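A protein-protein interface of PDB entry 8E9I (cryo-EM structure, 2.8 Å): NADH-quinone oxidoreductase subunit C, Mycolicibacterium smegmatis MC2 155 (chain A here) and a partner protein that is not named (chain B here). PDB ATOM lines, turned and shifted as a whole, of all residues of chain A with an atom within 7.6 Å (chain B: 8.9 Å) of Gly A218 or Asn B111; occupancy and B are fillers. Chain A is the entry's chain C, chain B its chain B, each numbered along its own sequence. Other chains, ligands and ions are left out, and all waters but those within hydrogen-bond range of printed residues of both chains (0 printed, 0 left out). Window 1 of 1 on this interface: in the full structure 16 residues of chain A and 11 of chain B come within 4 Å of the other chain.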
ATOM      1  N   PRO A 215      -2.345  -5.846  15.481  1.00  0.00           N
ATOM      2  CA  PRO A 215      -0.943  -5.451  15.340  1.00  0.00           C
ATOM      3  C   PRO A 215      -0.079  -6.630  14.933  1.00  0.00           C
ATOM      4  O   PRO A 215      -0.380  -7.787  15.224  1.00  0.00           O
ATOM      5  CB  PRO A 215      -0.575  -4.944  16.736  1.00  0.00           C
ATOM      6  CG  PRO A 215      -1.457  -5.709  17.639  1.00  0.00           C
ATOM      7  CD  PRO A 215      -2.754  -5.893  16.895  1.00  0.00           C
ATOM      8  N   LEU A 216       1.021  -6.317  14.249  1.00  0.00           N
ATOM      9  CA  LEU A 216       1.892  -7.373  13.750  1.00  0.00           C
ATOM     10  C   LEU A 216       2.408  -8.256  14.874  1.00  0.00           C
ATOM     11  O   LEU A 216       2.742  -9.419  14.640  1.00  0.00           O
ATOM     12  CB  LEU A 216       3.061  -6.771  12.978  1.00  0.00           C
ATOM     13  CG  LEU A 216       4.055  -7.779  12.401  1.00  0.00           C
ATOM     14  CD1 LEU A 216       3.372  -8.734  11.447  1.00  0.00           C
ATOM     15  CD2 LEU A 216       5.192  -7.060  11.706  1.00  0.00           C
ATOM     16  N   GLY A 217       2.484  -7.730  16.090  1.00  0.00           N
ATOM     17  CA  GLY A 217       2.931  -8.531  17.211  1.00  0.00           C
ATOM     18  C   GLY A 217       4.366  -8.993  17.126  1.00  0.00           C
ATOM     19  O   GLY A 217       4.676 -10.101  17.567  1.00  0.00           O
ATOM     20  N   GLY A 218       5.253  -8.177  16.568  1.00  0.00           N
ATOM     21  CA  GLY A 218       6.665  -8.475  16.578  1.00  0.00           C
ATOM     22  C   GLY A 218       7.347  -7.926  17.812  1.00  0.00           C
ATOM     23  O   GLY A 218       6.745  -7.266  18.657  1.00  0.00           O
ATOM     24  N   ILE A 219       8.642  -8.204  17.911  1.00  0.00           N
ATOM     25  CA  ILE A 219       9.447  -7.696  19.017  1.00  0.00           C
ATOM     26  C   ILE A 219      10.675  -6.997  18.449  1.00  0.00           C
ATOM     27  O   ILE A 219      11.099  -7.312  17.330  1.00  0.00           O
ATOM     28  CB  ILE A 219       9.840  -8.821  19.985  1.00  0.00           C
ATOM     29  CG1 ILE A 219      10.740  -9.843  19.295  1.00  0.00           C
ATOM     30  CG2 ILE A 219       8.608  -9.509  20.509  1.00  0.00           C
ATOM     31  CD1 ILE A 219      11.327 -10.840  20.243  1.00  0.00           C
ATOM     32  N   PRO A 220      11.272  -6.048  19.162  1.00  0.00           N
ATOM     33  CA  PRO A 220      12.482  -5.403  18.646  1.00  0.00           C
ATOM     34  C   PRO A 220      13.613  -6.402  18.456  1.00  0.00           C
ATOM     35  O   PRO A 220      13.826  -7.292  19.281  1.00  0.00           O
ATOM     36  CB  PRO A 220      12.815  -4.365  19.719  1.00  0.00           C
ATOM     37  CG  PRO A 220      11.541  -4.136  20.432  1.00  0.00           C
ATOM     38  CD  PRO A 220      10.846  -5.449  20.436  1.00  0.00           C
ATOM     39  N   VAL A 221      14.343  -6.238  17.359  1.00  0.00           N
ATOM     40  CA  VAL A 221      15.535  -7.032  17.100  1.00  0.00           C
ATOM     41  C   VAL A 221      16.692  -6.419  17.870  1.00  0.00           C
ATOM     42  O   VAL A 221      16.930  -5.211  17.787  1.00  0.00           O
ATOM     43  CB  VAL A 221      15.837  -7.082  15.600  1.00  0.00           C
ATOM     44  CG1 VAL A 221      17.063  -7.929  15.339  1.00  0.00           C
ATOM     45  CG2 VAL A 221      14.638  -7.603  14.841  1.00  0.00           C
ATOM     46  N   GLU A 222      17.414  -7.242  18.619  1.00  0.00           N
ATOM     47  CA  GLU A 222      18.450  -6.738  19.506  1.00  0.00           C
ATOM     48  C   GLU A 222      19.774  -6.572  18.773  1.00  0.00           C
ATOM     49  O   GLU A 222      20.083  -7.299  17.829  1.00  0.00           O
ATOM     50  CB  GLU A 222      18.634  -7.679  20.695  1.00  0.00           C
ATOM     51  N   ILE A 228      16.050  -2.610  16.865  1.00  0.00           N
ATOM     52  CA  ILE A 228      15.243  -2.186  15.726  1.00  0.00           C
ATOM     53  C   ILE A 228      13.800  -2.597  15.998  1.00  0.00           C
ATOM     54  O   ILE A 228      13.522  -3.793  16.118  1.00  0.00           O
ATOM     55  CB  ILE A 228      15.748  -2.798  14.412  1.00  0.00           C
ATOM     56  CG1 ILE A 228      17.205  -2.410  14.177  1.00  0.00           C
ATOM     57  CG2 ILE A 228      14.903  -2.327  13.249  1.00  0.00           C
ATOM     58  CD1 ILE A 228      17.801  -3.008  12.929  1.00  0.00           C
ATOM     59  N   PRO A 229      12.861  -1.665  16.096  1.00  0.00           N
ATOM     60  CA  PRO A 229      11.464  -2.045  16.284  1.00  0.00           C
ATOM     61  C   PRO A 229      10.943  -2.809  15.081  1.00  0.00           C
ATOM     62  O   PRO A 229      11.502  -2.705  13.980  1.00  0.00           O
ATOM     63  CB  PRO A 229      10.752  -0.696  16.436  1.00  0.00           C
ATOM     64  CG  PRO A 229      11.812   0.229  16.885  1.00  0.00           C
ATOM     65  CD  PRO A 229      13.035  -0.209  16.172  1.00  0.00           C
ATOM     66  N   PRO A 230       9.875  -3.582  15.246  1.00  0.00           N
ATOM     67  CA  PRO A 230       9.347  -4.369  14.130  1.00  0.00           C
ATOM     68  C   PRO A 230       9.018  -3.481  12.946  1.00  0.00           C
ATOM     69  O   PRO A 230       8.956  -2.251  13.079  1.00  0.00           O
ATOM     70  CB  PRO A 230       8.079  -5.008  14.712  1.00  0.00           C
ATOM     71  CG  PRO A 230       8.262  -4.960  16.177  1.00  0.00           C
ATOM     72  CD  PRO A 230       9.059  -3.736  16.461  1.00  0.00           C
ATOM     73  N   PRO A 231       8.812  -4.067  11.765  1.00  0.00           N
ATOM     74  CA  PRO A 231       8.509  -3.252  10.581  1.00  0.00           C
ATOM     75  C   PRO A 231       7.210  -2.473  10.673  1.00  0.00           C
ATOM     76  O   PRO A 231       7.085  -1.447   9.996  1.00  0.00           O
ATOM     77  CB  PRO A 231       8.452  -4.288   9.456  1.00  0.00           C
ATOM     78  CG  PRO A 231       8.083  -5.543  10.136  1.00  0.00           C
ATOM     79  CD  PRO A 231       8.801  -5.502  11.450  1.00  0.00           C
ATOM     80  N   ASP A 232       6.237  -2.919  11.463  1.00  0.00           N
ATOM     81  CA  ASP A 232       4.961  -2.220  11.518  1.00  0.00           C
ATOM     82  C   ASP A 232       5.038  -0.920  12.300  1.00  0.00           C
ATOM     83  O   ASP A 232       4.137  -0.088  12.177  1.00  0.00           O
ATOM     84  CB  ASP A 232       3.889  -3.109  12.139  1.00  0.00           C
ATOM     85  CG  ASP A 232       4.060  -3.265  13.631  1.00  0.00           C
ATOM     86  OD1 ASP A 232       5.216  -3.308  14.089  1.00  0.00           O
ATOM     87  OD2 ASP A 232       3.039  -3.334  14.347  1.00  0.00           O
ATOM     88  N   GLN A 233       6.079  -0.733  13.105  1.00  0.00           N
ATOM     89  CA  GLN A 233       6.218   0.501  13.865  1.00  0.00           C
ATOM     90  C   GLN A 233       6.999   1.550  13.090  1.00  0.00           C
ATOM     91  O   GLN A 233       6.692   2.742  13.171  1.00  0.00           O
ATOM     92  CB  GLN A 233       6.907   0.215  15.194  1.00  0.00           C
ATOM     93  CG  GLN A 233       6.193  -0.807  16.039  1.00  0.00           C
ATOM     94  CD  GLN A 233       6.833  -0.976  17.392  1.00  0.00           C
ATOM     95  OE1 GLN A 233       7.690  -0.193  17.786  1.00  0.00           O
ATOM     96  NE2 GLN A 233       6.418  -2.005  18.116  1.00  0.00           N
ATOM     97  N   ARG A 234       8.006   1.129  12.339  1.00  0.00           N
ATOM     98  CA  ARG A 234       8.865   2.069  11.651  1.00  0.00           C
ATOM     99  C   ARG A 234       8.170   2.629  10.419  1.00  0.00           C
ATOM    100  O   ARG A 234       7.137   2.131   9.970  1.00  0.00           O
ATOM    101  CB  ARG A 234      10.179   1.401  11.271  1.00  0.00           C
ATOM    102  CG  ARG A 234      10.857   0.719  12.446  1.00  0.00           C
ATOM    103  CD  ARG A 234      12.278   0.354  12.125  1.00  0.00           C
ATOM    104  NE  ARG A 234      12.401  -0.041  10.730  1.00  0.00           N
ATOM    105  CZ  ARG A 234      12.296  -1.284  10.286  1.00  0.00           C
ATOM    106  NH1 ARG A 234      12.061  -2.294  11.104  1.00  0.00           N
ATOM    107  NH2 ARG A 234      12.414  -1.517   8.983  1.00  0.00           N
ATOM    108  N   GLN B  78       3.461 -20.356  18.067  1.00  0.00           N
ATOM    109  CA  GLN B  78       2.883 -20.306  19.404  1.00  0.00           C
ATOM    110  C   GLN B  78       2.256 -21.642  19.763  1.00  0.00           C
ATOM    111  O   GLN B  78       2.473 -22.175  20.854  1.00  0.00           O
ATOM    112  CB  GLN B  78       1.843 -19.190  19.476  1.00  0.00           C
ATOM    113  CG  GLN B  78       2.412 -17.825  19.210  1.00  0.00           C
ATOM    114  CD  GLN B  78       3.266 -17.331  20.341  1.00  0.00           C
ATOM    115  OE1 GLN B  78       3.445 -18.016  21.340  1.00  0.00           O
ATOM    116  NE2 GLN B  78       3.818 -16.140  20.185  1.00  0.00           N
ATOM    117  N   VAL B 102      17.865 -19.535  12.182  1.00  0.00           N
ATOM    118  CA  VAL B 102      17.492 -18.244  12.741  1.00  0.00           C
ATOM    119  C   VAL B 102      16.101 -18.302  13.345  1.00  0.00           C
ATOM    120  O   VAL B 102      15.833 -17.658  14.366  1.00  0.00           O
ATOM    121  CB  VAL B 102      17.592 -17.147  11.669  1.00  0.00           C
ATOM    122  CG1 VAL B 102      19.028 -16.939  11.271  1.00  0.00           C
ATOM    123  CG2 VAL B 102      16.751 -17.498  10.464  1.00  0.00           C
ATOM    124  N   CYS B 103      15.193 -19.066  12.739  1.00  0.00           N
ATOM    125  CA  CYS B 103      13.853 -19.192  13.300  1.00  0.00           C
ATOM    126  C   CYS B 103      13.902 -19.776  14.703  1.00  0.00           C
ATOM    127  O   CYS B 103      13.304 -19.231  15.635  1.00  0.00           O
ATOM    128  CB  CYS B 103      12.982 -20.059  12.398  1.00  0.00           C
ATOM    129  SG  CYS B 103      12.409 -19.245  10.900  1.00  0.00           S
ATOM    130  N   SER B 106      16.248 -17.235  17.207  1.00  0.00           N
ATOM    131  CA  SER B 106      15.752 -15.921  17.589  1.00  0.00           C
ATOM    132  C   SER B 106      14.455 -15.516  16.907  1.00  0.00           C
ATOM    133  O   SER B 106      14.076 -14.351  17.020  1.00  0.00           O
ATOM    134  CB  SER B 106      16.829 -14.875  17.292  1.00  0.00           C
ATOM    135  OG  SER B 106      16.884 -14.603  15.905  1.00  0.00           O
ATOM    136  N   GLY B 107      13.762 -16.413  16.215  1.00  0.00           N
ATOM    137  CA  GLY B 107      12.609 -16.044  15.430  1.00  0.00           C
ATOM    138  C   GLY B 107      12.915 -15.735  13.985  1.00  0.00           C
ATOM    139  O   GLY B 107      12.000 -15.752  13.156  1.00  0.00           O
ATOM    140  N   GLY B 108      14.170 -15.460  13.658  1.00  0.00           N
ATOM    141  CA  GLY B 108      14.533 -15.239  12.275  1.00  0.00           C
ATOM    142  C   GLY B 108      13.744 -14.103  11.665  1.00  0.00           C
ATOM    143  O   GLY B 108      13.300 -13.177  12.349  1.00  0.00           O
ATOM    144  N   MET B 109      13.557 -14.184  10.349  1.00  0.00           N
ATOM    145  CA  MET B 109      12.842 -13.143   9.625  1.00  0.00           C
ATOM    146  C   MET B 109      11.409 -12.992  10.108  1.00  0.00           C
ATOM    147  O   MET B 109      10.826 -11.910   9.992  1.00  0.00           O
ATOM    148  CB  MET B 109      12.869 -13.470   8.139  1.00  0.00           C
ATOM    149  CG  MET B 109      12.170 -12.481   7.247  1.00  0.00           C
ATOM    150  SD  MET B 109      12.331 -12.990   5.532  1.00  0.00           S
ATOM    151  CE  MET B 109      11.279 -14.424   5.528  1.00  0.00           C
ATOM    152  N   PHE B 110      10.826 -14.056  10.651  1.00  0.00           N
ATOM    153  CA  PHE B 110       9.413 -14.066  11.009  1.00  0.00           C
ATOM    154  C   PHE B 110       9.200 -13.462  12.399  1.00  0.00           C
ATOM    155  O   PHE B 110       8.760 -14.112  13.342  1.00  0.00           O
ATOM    156  CB  PHE B 110       8.884 -15.489  10.921  1.00  0.00           C
ATOM    157  CG  PHE B 110       9.075 -16.103   9.578  1.00  0.00           C
ATOM    158  CD1 PHE B 110       8.502 -15.532   8.462  1.00  0.00           C
ATOM    159  CD2 PHE B 110       9.846 -17.233   9.420  1.00  0.00           C
ATOM    160  CE1 PHE B 110       8.679 -16.087   7.217  1.00  0.00           C
ATOM    161  CE2 PHE B 110      10.027 -17.791   8.176  1.00  0.00           C
ATOM    162  CZ  PHE B 110       9.446 -17.216   7.074  1.00  0.00           C
ATOM    163  N   ASN B 111       9.537 -12.177  12.499  1.00  0.00           N
ATOM    164  CA  ASN B 111       9.286 -11.388  13.702  1.00  0.00           C
ATOM    165  C   ASN B 111       7.803 -11.025  13.728  1.00  0.00           C
ATOM    166  O   ASN B 111       7.375  -9.958  13.286  1.00  0.00           O
ATOM    167  CB  ASN B 111      10.175 -10.156  13.713  1.00  0.00           C
ATOM    168  CG  ASN B 111      10.187  -9.459  15.048  1.00  0.00           C
ATOM    169  OD1 ASN B 111       9.586  -9.923  16.009  1.00  0.00           O
ATOM    170  ND2 ASN B 111      10.888  -8.342  15.117  1.00  0.00           N
ATOM    171  N   ASN B 112       7.008 -11.954  14.248  1.00  0.00           N
ATOM    172  CA  ASN B 112       5.564 -11.866  14.129  1.00  0.00           C
ATOM    173  C   ASN B 112       4.901 -12.381  15.394  1.00  0.00           C
ATOM    174  O   ASN B 112       5.554 -12.874  16.314  1.00  0.00           O
ATOM    175  CB  ASN B 112       5.052 -12.660  12.920  1.00  0.00           C
ATOM    176  N   TYR B 113       3.577 -12.243  15.422  1.00  0.00           N
ATOM    177  CA  TYR B 113       2.783 -12.809  16.504  1.00  0.00           C
ATOM    178  C   TYR B 113       2.880 -14.326  16.528  1.00  0.00           C
ATOM    179  O   TYR B 113       2.979 -14.935  17.597  1.00  0.00           O
ATOM    180  CB  TYR B 113       1.326 -12.383  16.341  1.00  0.00           C
ATOM    181  CG  TYR B 113       0.682 -12.972  15.110  1.00  0.00           C
ATOM    182  CD1 TYR B 113       0.912 -12.425  13.860  1.00  0.00           C
ATOM    183  CD2 TYR B 113      -0.129 -14.089  15.192  1.00  0.00           C
ATOM    184  CE1 TYR B 113       0.343 -12.960  12.735  1.00  0.00           C
ATOM    185  CE2 TYR B 113      -0.705 -14.629  14.071  1.00  0.00           C
ATOM    186  CZ  TYR B 113      -0.458 -14.066  12.843  1.00  0.00           C
ATOM    187  OH  TYR B 113      -1.030 -14.595  11.712  1.00  0.00           O
ATOM    188  N   ALA B 114       2.844 -14.957  15.355  1.00  0.00           N
ATOM    189  CA  ALA B 114       2.686 -16.400  15.289  1.00  0.00           C
ATOM    190  C   ALA B 114       3.905 -17.153  15.798  1.00  0.00           C
ATOM    191  O   ALA B 114       3.768 -18.300  16.226  1.00  0.00           O
ATOM    192  CB  ALA B 114       2.386 -16.822  13.852  1.00  0.00           C
ATOM    193  N   VAL B 115       5.082 -16.541  15.773  1.00  0.00           N
ATOM    194  CA  VAL B 115       6.333 -17.232  16.046  1.00  0.00           C
ATOM    195  C   VAL B 115       6.845 -16.807  17.412  1.00  0.00           C
ATOM    196  O   VAL B 115       6.763 -15.632  17.778  1.00  0.00           O
ATOM    197  CB  VAL B 115       7.381 -16.940  14.957  1.00  0.00           C
ATOM    198  CG1 VAL B 115       8.688 -17.611  15.292  1.00  0.00           C
ATOM    199  CG2 VAL B 115       6.872 -17.391  13.602  1.00  0.00           C
ATOM    200  N   VAL B 116       7.386 -17.770  18.160  1.00  0.00           N
ATOM    201  CA  VAL B 116       7.802 -17.520  19.538  1.00  0.00           C
ATOM    202  C   VAL B 116       9.014 -16.612  19.652  1.00  0.00           C
ATOM    203  O   VAL B 116       9.250 -16.050  20.728  1.00  0.00           O
ATOM    204  CB  VAL B 116       8.091 -18.861  20.237  1.00  0.00           C
ATOM    205  CG1 VAL B 116       8.712 -18.633  21.594  1.00  0.00           C
ATOM    206  CG2 VAL B 116       6.814 -19.655  20.374  1.00  0.00           C
ATOM    207  N   GLN B 117       9.778 -16.435  18.579  1.00  0.00           N
ATOM    208  CA  GLN B 117      10.986 -15.613  18.605  1.00  0.00           C
ATOM    209  C   GLN B 117      12.072 -16.249  19.469  1.00  0.00           C
ATOM    210  O   GLN B 117      12.602 -15.623  20.386  1.00  0.00           O
ATOM    211  CB  GLN B 117      10.687 -14.188  19.079  1.00  0.00           C
ATOM    212  CG  GLN B 117       9.550 -13.507  18.342  1.00  0.00           C
ATOM    213  CD  GLN B 117       9.736 -13.521  16.842  1.00  0.00           C
ATOM    214  OE1 GLN B 117      10.749 -13.058  16.329  1.00  0.00           O
ATOM    215  NE2 GLN B 117       8.756 -14.053  16.129  1.00  0.00           N
ATOM    216  N   GLY B 118      12.403 -17.500  19.174  1.00  0.00           N
ATOM    217  CA  GLY B 118      13.477 -18.178  19.866  1.00  0.00           C
ATOM    218  C   GLY B 118      12.970 -19.221  20.832  1.00  0.00           C
ATOM    219  O   GLY B 118      12.202 -18.910  21.743  1.00  0.00           O
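O of Ile A219 lies within hydrogen-bond range of ND2 of Asn B111, 2.5 Å away. The backbone NH (N) of Tyr B113 sits at hydrogen-bond distance from the backbone carbonyl oxygen (O) of Leu A216 (3.0 Å). N of Tyr B113 is in hydrogen-bond range of O of Gly A217, at 3.2 Å. O of Gly A217 lies close to O of Asn B112.
O of Tyr B113 lies within hydrogen-bond range of NE2 of Gln B78. O of Phe B110 lies within hydrogen-bond range of NE2 of Gln B117 (2.8 Å). The side-chain amide oxygen (OD1) of Asn B111 lies close to the side-chain amide oxygen (OE1) of Gln B117, at 3.4 Å. The backbone NH (N) of Asn B112 lies close to the side-chain amide nitrogen (NE2) of Gln B117, 3.3 Å away. NE2 of Gln B117 is in hydrogen-bond range of O of Val B115, 3.0 Å away. N of Val A221 lies within hydrogen-bond range of O of Ile A228, 2.9 Å away.
Among the printed residues, merely in contact across the chains: Leu A216 with Asn B111, Leu A216 with Asn B112, Gly A218 with Asn B111, Ile A219 with Gln B117 and Val A221 with Asn B111.
Of the printed residues of chain B, Leu A216 touches Asn B111, Asn B112 and Tyr B113. Gly A217 touches two residues of chain B. Gly A218 touches just one residue of chain B: Asn B111. Of chain A, only Leu A216 (3.96 Å), Gly A218 (3.3 Å), Ile A219 (2.5 Å) and Val A221 (3.8 Å) come within 4 Å of Asn B111. Printed residues of chain A within 4 Å of Asn B112: Leu A216 and Gly A217. Printed residues of chain A within 4 Å of Tyr B113: Leu A216 (3.0 Å) and Gly A217 (3.2 Å). Ala B114 touches none of the printed residues of chain A. Val B115 touches none of the printed residues of chain A. The nearest printed residue of chain A that does not touch Asn B112 is Gly A218 (4.2 Å).
Hydrophobic or aromatic side chains of chain A that line the printed part of chain B: Leu A216, Ile A219 and Val A221. Printed residues of chain B that touch a printed residue of chain A: Asn B111, Asn B112, Tyr B113 and Gln B117. Hydrophobic or aromatic side chains of chain B that line the printed part of chain A: Tyr B113. Among the printed residues, no Asp or Glu carboxylate lies within 4 Å of a Lys or Arg side-chain nitrogen of the other chain.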
